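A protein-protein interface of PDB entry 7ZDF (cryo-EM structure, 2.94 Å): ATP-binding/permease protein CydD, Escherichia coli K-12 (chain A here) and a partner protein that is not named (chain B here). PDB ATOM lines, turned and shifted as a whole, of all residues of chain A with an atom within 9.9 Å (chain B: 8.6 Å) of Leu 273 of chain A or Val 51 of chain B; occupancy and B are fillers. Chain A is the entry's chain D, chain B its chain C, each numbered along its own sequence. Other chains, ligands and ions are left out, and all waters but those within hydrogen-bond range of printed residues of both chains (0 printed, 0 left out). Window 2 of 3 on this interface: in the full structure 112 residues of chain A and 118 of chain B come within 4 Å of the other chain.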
ATOM      1  N   MET A  54      19.942 -18.877  24.175  1.00  0.00           N
ATOM      2  CA  MET A  54      21.143 -18.666  23.372  1.00  0.00           C
ATOM      3  C   MET A  54      22.366 -18.400  24.240  1.00  0.00           C
ATOM      4  O   MET A  54      23.415 -19.022  24.045  1.00  0.00           O
ATOM      5  CB  MET A  54      20.928 -17.510  22.396  1.00  0.00           C
ATOM      6  CG  MET A  54      19.845 -17.758  21.365  1.00  0.00           C
ATOM      7  SD  MET A  54      20.040 -19.330  20.508  1.00  0.00           S
ATOM      8  CE  MET A  54      20.976 -18.812  19.072  1.00  0.00           C
ATOM      9  N   ALA A 265       6.612 -18.690  12.229  1.00  0.00           N
ATOM     10  CA  ALA A 265       7.514 -19.757  12.645  1.00  0.00           C
ATOM     11  C   ALA A 265       8.370 -20.251  11.486  1.00  0.00           C
ATOM     12  O   ALA A 265       9.573 -20.485  11.652  1.00  0.00           O
ATOM     13  CB  ALA A 265       6.717 -20.909  13.252  1.00  0.00           C
ATOM     14  N   VAL A 266       7.768 -20.427  10.308  1.00  0.00           N
ATOM     15  CA  VAL A 266       8.525 -20.891   9.149  1.00  0.00           C
ATOM     16  C   VAL A 266       9.556 -19.852   8.725  1.00  0.00           C
ATOM     17  O   VAL A 266      10.709 -20.189   8.433  1.00  0.00           O
ATOM     18  CB  VAL A 266       7.572 -21.248   7.995  1.00  0.00           C
ATOM     19  CG1 VAL A 266       8.349 -21.450   6.709  1.00  0.00           C
ATOM     20  CG2 VAL A 266       6.788 -22.502   8.332  1.00  0.00           C
ATOM     21  N   TYR A 267       9.164 -18.578   8.681  1.00  0.00           N
ATOM     22  CA  TYR A 267      10.094 -17.538   8.254  1.00  0.00           C
ATOM     23  C   TYR A 267      11.262 -17.409   9.222  1.00  0.00           C
ATOM     24  O   TYR A 267      12.427 -17.448   8.814  1.00  0.00           O
ATOM     25  CB  TYR A 267       9.370 -16.200   8.116  1.00  0.00           C
ATOM     26  CG  TYR A 267      10.306 -15.015   8.148  1.00  0.00           C
ATOM     27  CD1 TYR A 267      11.180 -14.767   7.102  1.00  0.00           C
ATOM     28  CD2 TYR A 267      10.323 -14.149   9.231  1.00  0.00           C
ATOM     29  CE1 TYR A 267      12.041 -13.691   7.130  1.00  0.00           C
ATOM     30  CE2 TYR A 267      11.181 -13.070   9.266  1.00  0.00           C
ATOM     31  CZ  TYR A 267      12.037 -12.846   8.215  1.00  0.00           C
ATOM     32  OH  TYR A 267      12.891 -11.772   8.248  1.00  0.00           O
ATOM     33  N   PHE A 268      10.968 -17.256  10.513  1.00  0.00           N
ATOM     34  CA  PHE A 268      12.038 -17.090  11.491  1.00  0.00           C
ATOM     35  C   PHE A 268      12.834 -18.376  11.665  1.00  0.00           C
ATOM     36  O   PHE A 268      14.059 -18.335  11.818  1.00  0.00           O
ATOM     37  CB  PHE A 268      11.465 -16.630  12.827  1.00  0.00           C
ATOM     38  CG  PHE A 268      11.257 -15.150  12.914  1.00  0.00           C
ATOM     39  CD1 PHE A 268       9.984 -14.614  12.878  1.00  0.00           C
ATOM     40  CD2 PHE A 268      12.336 -14.294  13.019  1.00  0.00           C
ATOM     41  CE1 PHE A 268       9.791 -13.254  12.953  1.00  0.00           C
ATOM     42  CE2 PHE A 268      12.148 -12.932  13.095  1.00  0.00           C
ATOM     43  CZ  PHE A 268      10.872 -12.412  13.060  1.00  0.00           C
ATOM     44  N   GLY A 269      12.158 -19.525  11.644  1.00  0.00           N
ATOM     45  CA  GLY A 269      12.860 -20.783  11.832  1.00  0.00           C
ATOM     46  C   GLY A 269      13.874 -21.058  10.740  1.00  0.00           C
ATOM     47  O   GLY A 269      14.998 -21.482  11.017  1.00  0.00           O
ATOM     48  N   PHE A 270      13.496 -20.820   9.484  1.00  0.00           N
ATOM     49  CA  PHE A 270      14.418 -21.025   8.377  1.00  0.00           C
ATOM     50  C   PHE A 270      15.390 -19.868   8.203  1.00  0.00           C
ATOM     51  O   PHE A 270      16.407 -20.030   7.521  1.00  0.00           O
ATOM     52  CB  PHE A 270      13.643 -21.249   7.078  1.00  0.00           C
ATOM     53  CG  PHE A 270      13.114 -22.643   6.928  1.00  0.00           C
ATOM     54  CD1 PHE A 270      11.811 -22.944   7.281  1.00  0.00           C
ATOM     55  CD2 PHE A 270      13.922 -23.655   6.447  1.00  0.00           C
ATOM     56  CE1 PHE A 270      11.324 -24.227   7.149  1.00  0.00           C
ATOM     57  CE2 PHE A 270      13.440 -24.940   6.313  1.00  0.00           C
ATOM     58  CZ  PHE A 270      12.138 -25.225   6.665  1.00  0.00           C
ATOM     59  N   SER A 271      15.103 -18.709   8.796  1.00  0.00           N
ATOM     60  CA  SER A 271      16.063 -17.612   8.757  1.00  0.00           C
ATOM     61  C   SER A 271      17.250 -17.883   9.670  1.00  0.00           C
ATOM     62  O   SER A 271      18.367 -17.441   9.380  1.00  0.00           O
ATOM     63  CB  SER A 271      15.380 -16.302   9.145  1.00  0.00           C
ATOM     64  OG  SER A 271      16.187 -15.189   8.811  1.00  0.00           O
ATOM     65  N   TYR A 272      17.029 -18.603  10.772  1.00  0.00           N
ATOM     66  CA  TYR A 272      18.139 -19.010  11.626  1.00  0.00           C
ATOM     67  C   TYR A 272      18.987 -20.076  10.944  1.00  0.00           C
ATOM     68  O   TYR A 272      20.210 -20.115  11.124  1.00  0.00           O
ATOM     69  CB  TYR A 272      17.615 -19.522  12.966  1.00  0.00           C
ATOM     70  CG  TYR A 272      16.815 -18.505  13.745  1.00  0.00           C
ATOM     71  CD1 TYR A 272      17.245 -17.193  13.858  1.00  0.00           C
ATOM     72  CD2 TYR A 272      15.630 -18.860  14.372  1.00  0.00           C
ATOM     73  CE1 TYR A 272      16.516 -16.262  14.568  1.00  0.00           C
ATOM     74  CE2 TYR A 272      14.894 -17.938  15.084  1.00  0.00           C
ATOM     75  CZ  TYR A 272      15.342 -16.641  15.180  1.00  0.00           C
ATOM     76  OH  TYR A 272      14.612 -15.718  15.889  1.00  0.00           O
ATOM     77  N   LEU A 273      18.353 -20.951  10.163  1.00  0.00           N
ATOM     78  CA  LEU A 273      19.068 -21.991   9.437  1.00  0.00           C
ATOM     79  C   LEU A 273      19.795 -21.461   8.209  1.00  0.00           C
ATOM     80  O   LEU A 273      20.570 -22.207   7.601  1.00  0.00           O
ATOM     81  CB  LEU A 273      18.099 -23.101   9.026  1.00  0.00           C
ATOM     82  CG  LEU A 273      17.368 -23.818  10.161  1.00  0.00           C
ATOM     83  CD1 LEU A 273      16.389 -24.838   9.608  1.00  0.00           C
ATOM     84  CD2 LEU A 273      18.357 -24.479  11.103  1.00  0.00           C
ATOM     85  N   GLY A 274      19.566 -20.206   7.829  1.00  0.00           N
ATOM     86  CA  GLY A 274      20.282 -19.591   6.733  1.00  0.00           C
ATOM     87  C   GLY A 274      19.649 -19.728   5.367  1.00  0.00           C
ATOM     88  O   GLY A 274      20.186 -19.172   4.401  1.00  0.00           O
ATOM     89  N   GLU A 275      18.536 -20.455   5.244  1.00  0.00           N
ATOM     90  CA  GLU A 275      17.885 -20.581   3.944  1.00  0.00           C
ATOM     91  C   GLU A 275      17.354 -19.239   3.456  1.00  0.00           C
ATOM     92  O   GLU A 275      17.482 -18.905   2.273  1.00  0.00           O
ATOM     93  CB  GLU A 275      16.758 -21.610   4.013  1.00  0.00           C
ATOM     94  CG  GLU A 275      17.178 -22.935   4.609  1.00  0.00           C
ATOM     95  CD  GLU A 275      16.489 -24.115   3.953  1.00  0.00           C
ATOM     96  OE1 GLU A 275      16.419 -25.189   4.585  1.00  0.00           O
ATOM     97  OE2 GLU A 275      16.022 -23.967   2.804  1.00  0.00           O
ATOM     98  N   LEU A 276      16.757 -18.459   4.350  1.00  0.00           N
ATOM     99  CA  LEU A 276      16.243 -17.139   4.018  1.00  0.00           C
ATOM    100  C   LEU A 276      17.210 -16.072   4.513  1.00  0.00           C
ATOM    101  O   LEU A 276      17.832 -16.224   5.569  1.00  0.00           O
ATOM    102  CB  LEU A 276      14.860 -16.919   4.633  1.00  0.00           C
ATOM    103  CG  LEU A 276      13.823 -18.013   4.388  1.00  0.00           C
ATOM    104  CD1 LEU A 276      12.490 -17.634   5.006  1.00  0.00           C
ATOM    105  CD2 LEU A 276      13.666 -18.276   2.902  1.00  0.00           C
ATOM    106  N   ASP A 277      17.337 -14.991   3.739  1.00  0.00           N
ATOM    107  CA  ASP A 277      18.230 -13.903   4.117  1.00  0.00           C
ATOM    108  C   ASP A 277      17.589 -12.534   3.911  1.00  0.00           C
ATOM    109  O   ASP A 277      18.309 -11.542   3.749  1.00  0.00           O
ATOM    110  CB  ASP A 277      19.544 -13.983   3.332  1.00  0.00           C
ATOM    111  CG  ASP A 277      20.742 -13.540   4.152  1.00  0.00           C
ATOM    112  OD1 ASP A 277      21.847 -14.074   3.924  1.00  0.00           O
ATOM    113  OD2 ASP A 277      20.578 -12.661   5.024  1.00  0.00           O
ATOM    114  N   HIS A 280      15.175  -8.615   7.390  1.00  0.00           N
ATOM    115  CA  HIS A 280      15.870  -7.858   8.416  1.00  0.00           C
ATOM    116  C   HIS A 280      16.607  -6.691   7.770  1.00  0.00           C
ATOM    117  O   HIS A 280      16.618  -6.527   6.547  1.00  0.00           O
ATOM    118  CB  HIS A 280      16.827  -8.757   9.201  1.00  0.00           C
ATOM    119  CG  HIS A 280      17.639  -9.671   8.340  1.00  0.00           C
ATOM    120  ND1 HIS A 280      17.357 -11.014   8.207  1.00  0.00           N
ATOM    121  CD2 HIS A 280      18.729  -9.439   7.571  1.00  0.00           C
ATOM    122  CE1 HIS A 280      18.236 -11.568   7.391  1.00  0.00           C
ATOM    123  NE2 HIS A 280      19.079 -10.634   6.991  1.00  0.00           N
ATOM    124  N   VAL A 285      19.055 -11.718  12.182  1.00  0.00           N
ATOM    125  CA  VAL A 285      17.866 -12.059  12.956  1.00  0.00           C
ATOM    126  C   VAL A 285      18.291 -12.722  14.257  1.00  0.00           C
ATOM    127  O   VAL A 285      19.097 -13.660  14.262  1.00  0.00           O
ATOM    128  CB  VAL A 285      16.928 -12.968  12.146  1.00  0.00           C
ATOM    129  CG1 VAL A 285      16.205 -12.165  11.083  1.00  0.00           C
ATOM    130  CG2 VAL A 285      17.708 -14.101  11.507  1.00  0.00           C
ATOM    131  N   PHE B  42      10.086 -24.785  17.614  1.00  0.00           N
ATOM    132  CA  PHE B  42      10.787 -24.801  16.334  1.00  0.00           C
ATOM    133  C   PHE B  42      11.722 -23.606  16.190  1.00  0.00           C
ATOM    134  O   PHE B  42      12.799 -23.723  15.594  1.00  0.00           O
ATOM    135  CB  PHE B  42       9.777 -24.837  15.189  1.00  0.00           C
ATOM    136  CG  PHE B  42      10.401 -24.785  13.827  1.00  0.00           C
ATOM    137  CD1 PHE B  42      11.138 -25.852  13.349  1.00  0.00           C
ATOM    138  CD2 PHE B  42      10.243 -23.672  13.022  1.00  0.00           C
ATOM    139  CE1 PHE B  42      11.710 -25.809  12.094  1.00  0.00           C
ATOM    140  CE2 PHE B  42      10.814 -23.624  11.767  1.00  0.00           C
ATOM    141  CZ  PHE B  42      11.548 -24.694  11.303  1.00  0.00           C
ATOM    142  N   LEU B  43      11.325 -22.446  16.714  1.00  0.00           N
ATOM    143  CA  LEU B  43      12.199 -21.278  16.667  1.00  0.00           C
ATOM    144  C   LEU B  43      13.451 -21.494  17.505  1.00  0.00           C
ATOM    145  O   LEU B  43      14.572 -21.256  17.042  1.00  0.00           O
ATOM    146  CB  LEU B  43      11.448 -20.036  17.143  1.00  0.00           C
ATOM    147  CG  LEU B  43      10.830 -19.161  16.060  1.00  0.00           C
ATOM    148  CD1 LEU B  43       9.687 -19.889  15.407  1.00  0.00           C
ATOM    149  CD2 LEU B  43      10.356 -17.855  16.655  1.00  0.00           C
ATOM    150  N   ALA B  45      14.651 -24.320  18.567  1.00  0.00           N
ATOM    151  CA  ALA B  45      15.414 -25.465  18.087  1.00  0.00           C
ATOM    152  C   ALA B  45      16.252 -25.103  16.869  1.00  0.00           C
ATOM    153  O   ALA B  45      17.394 -25.553  16.742  1.00  0.00           O
ATOM    154  CB  ALA B  45      14.478 -26.628  17.762  1.00  0.00           C
ATOM    155  N   SER B  46      15.698 -24.297  15.963  1.00  0.00           N
ATOM    156  CA  SER B  46      16.447 -23.882  14.784  1.00  0.00           C
ATOM    157  C   SER B  46      17.459 -22.790  15.105  1.00  0.00           C
ATOM    158  O   SER B  46      18.461 -22.655  14.394  1.00  0.00           O
ATOM    159  CB  SER B  46      15.487 -23.409  13.694  1.00  0.00           C
ATOM    160  OG  SER B  46      14.561 -22.470  14.204  1.00  0.00           O
ATOM    161  N   ALA B  47      17.220 -22.006  16.157  1.00  0.00           N
ATOM    162  CA  ALA B  47      18.173 -20.966  16.527  1.00  0.00           C
ATOM    163  C   ALA B  47      19.448 -21.563  17.107  1.00  0.00           C
ATOM    164  O   ALA B  47      20.554 -21.151  16.741  1.00  0.00           O
ATOM    165  CB  ALA B  47      17.536 -19.998  17.521  1.00  0.00           C
ATOM    166  N   VAL B  48      19.317 -22.534  18.014  1.00  0.00           N
ATOM    167  CA  VAL B  48      20.500 -23.167  18.585  1.00  0.00           C
ATOM    168  C   VAL B  48      21.222 -24.006  17.539  1.00  0.00           C
ATOM    169  O   VAL B  48      22.445 -24.169  17.603  1.00  0.00           O
ATOM    170  CB  VAL B  48      20.126 -23.999  19.827  1.00  0.00           C
ATOM    171  CG1 VAL B  48      19.388 -23.137  20.834  1.00  0.00           C
ATOM    172  CG2 VAL B  48      19.284 -25.200  19.442  1.00  0.00           C
ATOM    173  N   ALA B  49      20.489 -24.555  16.568  1.00  0.00           N
ATOM    174  CA  ALA B  49      21.136 -25.282  15.481  1.00  0.00           C
ATOM    175  C   ALA B  49      21.951 -24.343  14.602  1.00  0.00           C
ATOM    176  O   ALA B  49      23.103 -24.639  14.267  1.00  0.00           O
ATOM    177  CB  ALA B  49      20.094 -26.028  14.653  1.00  0.00           C
ATOM    178  N   GLY B  50      21.372 -23.206  14.223  1.00  0.00           N
ATOM    179  CA  GLY B  50      22.094 -22.241  13.423  1.00  0.00           C
ATOM    180  C   GLY B  50      22.318 -22.721  11.998  1.00  0.00           C
ATOM    181  O   GLY B  50      21.657 -23.634  11.497  1.00  0.00           O
ATOM    182  N   VAL B  51      23.282 -22.073  11.339  1.00  0.00           N
ATOM    183  CA  VAL B  51      23.645 -22.462   9.981  1.00  0.00           C
ATOM    184  C   VAL B  51      24.308 -23.835   9.974  1.00  0.00           C
ATOM    185  O   VAL B  51      24.183 -24.588   9.000  1.00  0.00           O
ATOM    186  CB  VAL B  51      24.549 -21.389   9.349  1.00  0.00           C
ATOM    187  CG1 VAL B  51      24.870 -21.734   7.903  1.00  0.00           C
ATOM    188  CG2 VAL B  51      23.888 -20.022   9.441  1.00  0.00           C
ATOM    189  N   ALA B  52      25.018 -24.183  11.050  1.00  0.00           N
ATOM    190  CA  ALA B  52      25.683 -25.481  11.115  1.00  0.00           C
ATOM    191  C   ALA B  52      24.678 -26.625  11.085  1.00  0.00           C
ATOM    192  O   ALA B  52      24.923 -27.661  10.456  1.00  0.00           O
ATOM    193  CB  ALA B  52      26.550 -25.562  12.370  1.00  0.00           C
ATOM    194  N   GLY B  53      23.543 -26.461  11.758  1.00  0.00           N
ATOM    195  CA  GLY B  53      22.538 -27.504  11.821  1.00  0.00           C
ATOM    196  C   GLY B  53      21.530 -27.435  10.692  1.00  0.00           C
ATOM    197  O   GLY B  53      20.449 -28.025  10.781  1.00  0.00           O
ATOM    198  N   LEU B  54      21.873 -26.706   9.629  1.00  0.00           N
ATOM    199  CA  LEU B  54      20.953 -26.536   8.507  1.00  0.00           C
ATOM    200  C   LEU B  54      20.618 -27.869   7.849  1.00  0.00           C
ATOM    201  O   LEU B  54      19.449 -28.159   7.570  1.00  0.00           O
ATOM    202  CB  LEU B  54      21.554 -25.570   7.487  1.00  0.00           C
ATOM    203  CG  LEU B  54      20.853 -25.477   6.131  1.00  0.00           C
ATOM    204  CD1 LEU B  54      19.394 -25.104   6.302  1.00  0.00           C
ATOM    205  CD2 LEU B  54      21.563 -24.474   5.232  1.00  0.00           C
ATOM    206  N   TYR B  55      21.630 -28.691   7.593  1.00  0.00           N
ATOM    207  CA  TYR B  55      21.445 -29.922   6.836  1.00  0.00           C
ATOM    208  C   TYR B  55      21.218 -31.142   7.718  1.00  0.00           C
ATOM    209  O   TYR B  55      21.123 -32.256   7.192  1.00  0.00           O
ATOM    210  CB  TYR B  55      22.651 -30.161   5.923  1.00  0.00           C
ATOM    211  CG  TYR B  55      22.493 -29.566   4.541  1.00  0.00           C
ATOM    212  CD1 TYR B  55      21.901 -30.289   3.516  1.00  0.00           C
ATOM    213  CD2 TYR B  55      22.933 -28.278   4.265  1.00  0.00           C
ATOM    214  CE1 TYR B  55      21.753 -29.750   2.252  1.00  0.00           C
ATOM    215  CE2 TYR B  55      22.789 -27.729   3.004  1.00  0.00           C
ATOM    216  CZ  TYR B  55      22.198 -28.469   2.002  1.00  0.00           C
ATOM    217  OH  TYR B  55      22.053 -27.927   0.746  1.00  0.00           O
ATOM    218  N   SER B  56      21.130 -30.968   9.033  1.00  0.00           N
ATOM    219  CA  SER B  56      20.914 -32.068   9.966  1.00  0.00           C
ATOM    220  C   SER B  56      19.865 -31.689  11.002  1.00  0.00           C
ATOM    221  O   SER B  56      20.040 -31.890  12.207  1.00  0.00           O
ATOM    222  CB  SER B  56      22.221 -32.472  10.640  1.00  0.00           C
ATOM    223  OG  SER B  56      22.708 -31.433  11.470  1.00  0.00           O
ATOM    224  N   PHE B  57      18.747 -31.128  10.542  1.00  0.00           N
ATOM    225  CA  PHE B  57      17.686 -30.690  11.439  1.00  0.00           C
ATOM    226  C   PHE B  57      16.385 -31.461  11.283  1.00  0.00           C
ATOM    227  O   PHE B  57      15.657 -31.611  12.266  1.00  0.00           O
ATOM    228  CB  PHE B  57      17.402 -29.195  11.242  1.00  0.00           C
ATOM    229  CG  PHE B  57      16.529 -28.606  12.308  1.00  0.00           C
ATOM    230  CD1 PHE B  57      16.971 -28.533  13.617  1.00  0.00           C
ATOM    231  CD2 PHE B  57      15.265 -28.132  12.006  1.00  0.00           C
ATOM    232  CE1 PHE B  57      16.171 -27.997  14.602  1.00  0.00           C
ATOM    233  CE2 PHE B  57      14.462 -27.594  12.989  1.00  0.00           C
ATOM    234  CZ  PHE B  57      14.915 -27.526  14.287  1.00  0.00           C
ATOM    235  N   ASN B  58      16.076 -31.951  10.080  1.00  0.00           N
ATOM    236  CA  ASN B  58      14.873 -32.742   9.816  1.00  0.00           C
ATOM    237  C   ASN B  58      13.611 -31.956  10.192  1.00  0.00           C
ATOM    238  O   ASN B  58      12.874 -32.289  11.123  1.00  0.00           O
ATOM    239  CB  ASN B  58      14.931 -34.092  10.543  1.00  0.00           C
ATOM    240  CG  ASN B  58      13.708 -34.951  10.279  1.00  0.00           C
ATOM    241  OD1 ASN B  58      13.396 -35.271   9.132  1.00  0.00           O
ATOM    242  ND2 ASN B  58      13.004 -35.321  11.341  1.00  0.00           N
ATOM    243  N   TYR B  59      13.398 -30.877   9.444  1.00  0.00           N
ATOM    244  CA  TYR B  59      12.231 -30.025   9.636  1.00  0.00           C
ATOM    245  C   TYR B  59      10.977 -30.579   8.974  1.00  0.00           C
ATOM    246  O   TYR B  59       9.922 -29.944   9.060  1.00  0.00           O
ATOM    247  CB  TYR B  59      12.510 -28.621   9.093  1.00  0.00           C
ATOM    248  CG  TYR B  59      13.030 -28.607   7.674  1.00  0.00           C
ATOM    249  CD1 TYR B  59      12.156 -28.635   6.595  1.00  0.00           C
ATOM    250  CD2 TYR B  59      14.393 -28.564   7.411  1.00  0.00           C
ATOM    251  CE1 TYR B  59      12.623 -28.622   5.296  1.00  0.00           C
ATOM    252  CE2 TYR B  59      14.870 -28.552   6.113  1.00  0.00           C
ATOM    253  CZ  TYR B  59      13.980 -28.581   5.060  1.00  0.00           C
ATOM    254  OH  TYR B  59      14.445 -28.567   3.766  1.00  0.00           O
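O of Phe 42 of chain B sits at hydrogen-bond distance from OG of Ser 46 of chain B, 2.6 Å away. The backbone carbonyl oxygen (O) of Leu 43 of chain B sits at hydrogen-bond distance from the side-chain hydroxyl (OG) of Ser 46 of chain B, 3.1 Å away. O of Phe 270 of chain A lies within hydrogen-bond range of N of Glu 275 of chain A, 3.1 Å away.
Of the 16 printed residues of chain A, 7 touch a printed residue of chain B. Printed residues of chain A that touch a printed residue of chain B: Met 54, Ala 265, Gly 269, Phe 270, Tyr 272, Leu 273 and Glu 275. Printed residues of chain B that touch a printed residue of chain A: Phe 42, Leu 43, Ser 46, Ala 47, Val 48, Gly 50, Val 51, Leu 54 and Tyr 59. Among the printed residues, 18 pairs touch across the chains.
O of Ala 47 of chain B touches CE of Met 54 of chain A, 3.3 Å away. CG1 of Val 48 of chain B touches SD of Met 54 of chain A, 3.9 Å away. Phe 42 of chain B touches Ala 265 of chain A. CA of Ala 265 of chain A touches CD1 of Leu 43 of chain B, 3.5 Å away. Phe 270 of chain A touches Tyr 59 of chain B (CZ to CD1, 3.4 Å). Leu 43 of chain B touches Tyr 272 of chain A (O to CD2, 3.7 Å). Tyr 272 of chain A touches Ser 46 of chain B. Ala 47 of chain B touches Tyr 272 of chain A. O of Tyr 272 of chain A touches N of Val 51 of chain B (3.6 Å). Leu 273 of chain A touches Val 51 of chain B.
OG of Ser 46 of chain B lies close to O of Gly 269 of chain A, at 3.4 Å.
Of chain B, only Ser 46 (3.8 Å), Gly 50 (3.4 Å), Val 51 (3.9 Å) and Leu 54 (3.4 Å) come within 4 Å of Leu 273 of chain A. Of chain A, only Tyr 272 (3.6 Å) and Leu 273 (3.9 Å) come within 4 Å of Val 51 of chain B. Of the printed residues of chain A, Gly 50 of chain B touches Tyr 272 and Leu 273. No residue of chain A comes within 4 Å of Ala 52 of chain B. Gly 53 of chain B touches none of the printed residues of chain A. Leu 54 of chain B touches just these residues of chain A: Leu 273 and Glu 275. Printed residues of chain A within 4 Å of Phe 42 of chain B: Ala 265 and Gly 269. Of the printed residues of chain B, Gly 269 of chain A touches Phe 42 (3.5 Å) and Ser 46 (3.3 Å). Printed residues of chain B within 4 Å of Tyr 272 of chain A: Leu 43, Ser 46, Ala 47, Gly 50 and Val 51. Of the printed residues of chain B, Met 54 of chain A touches Ala 47 and Val 48. Of the printed residues of chain B, Ala 265 of chain A touches Phe 42 and Leu 43. Leu 276 of chain A touches none of the printed residues of chain B. The nearest residue of chain B that does not touch Leu 273 of chain A is Gly 53 of chain B (4.1 Å). The nearest printed residue of chain A that does not touch Val 48 of chain B is Tyr 272 of chain A (6.1 Å).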
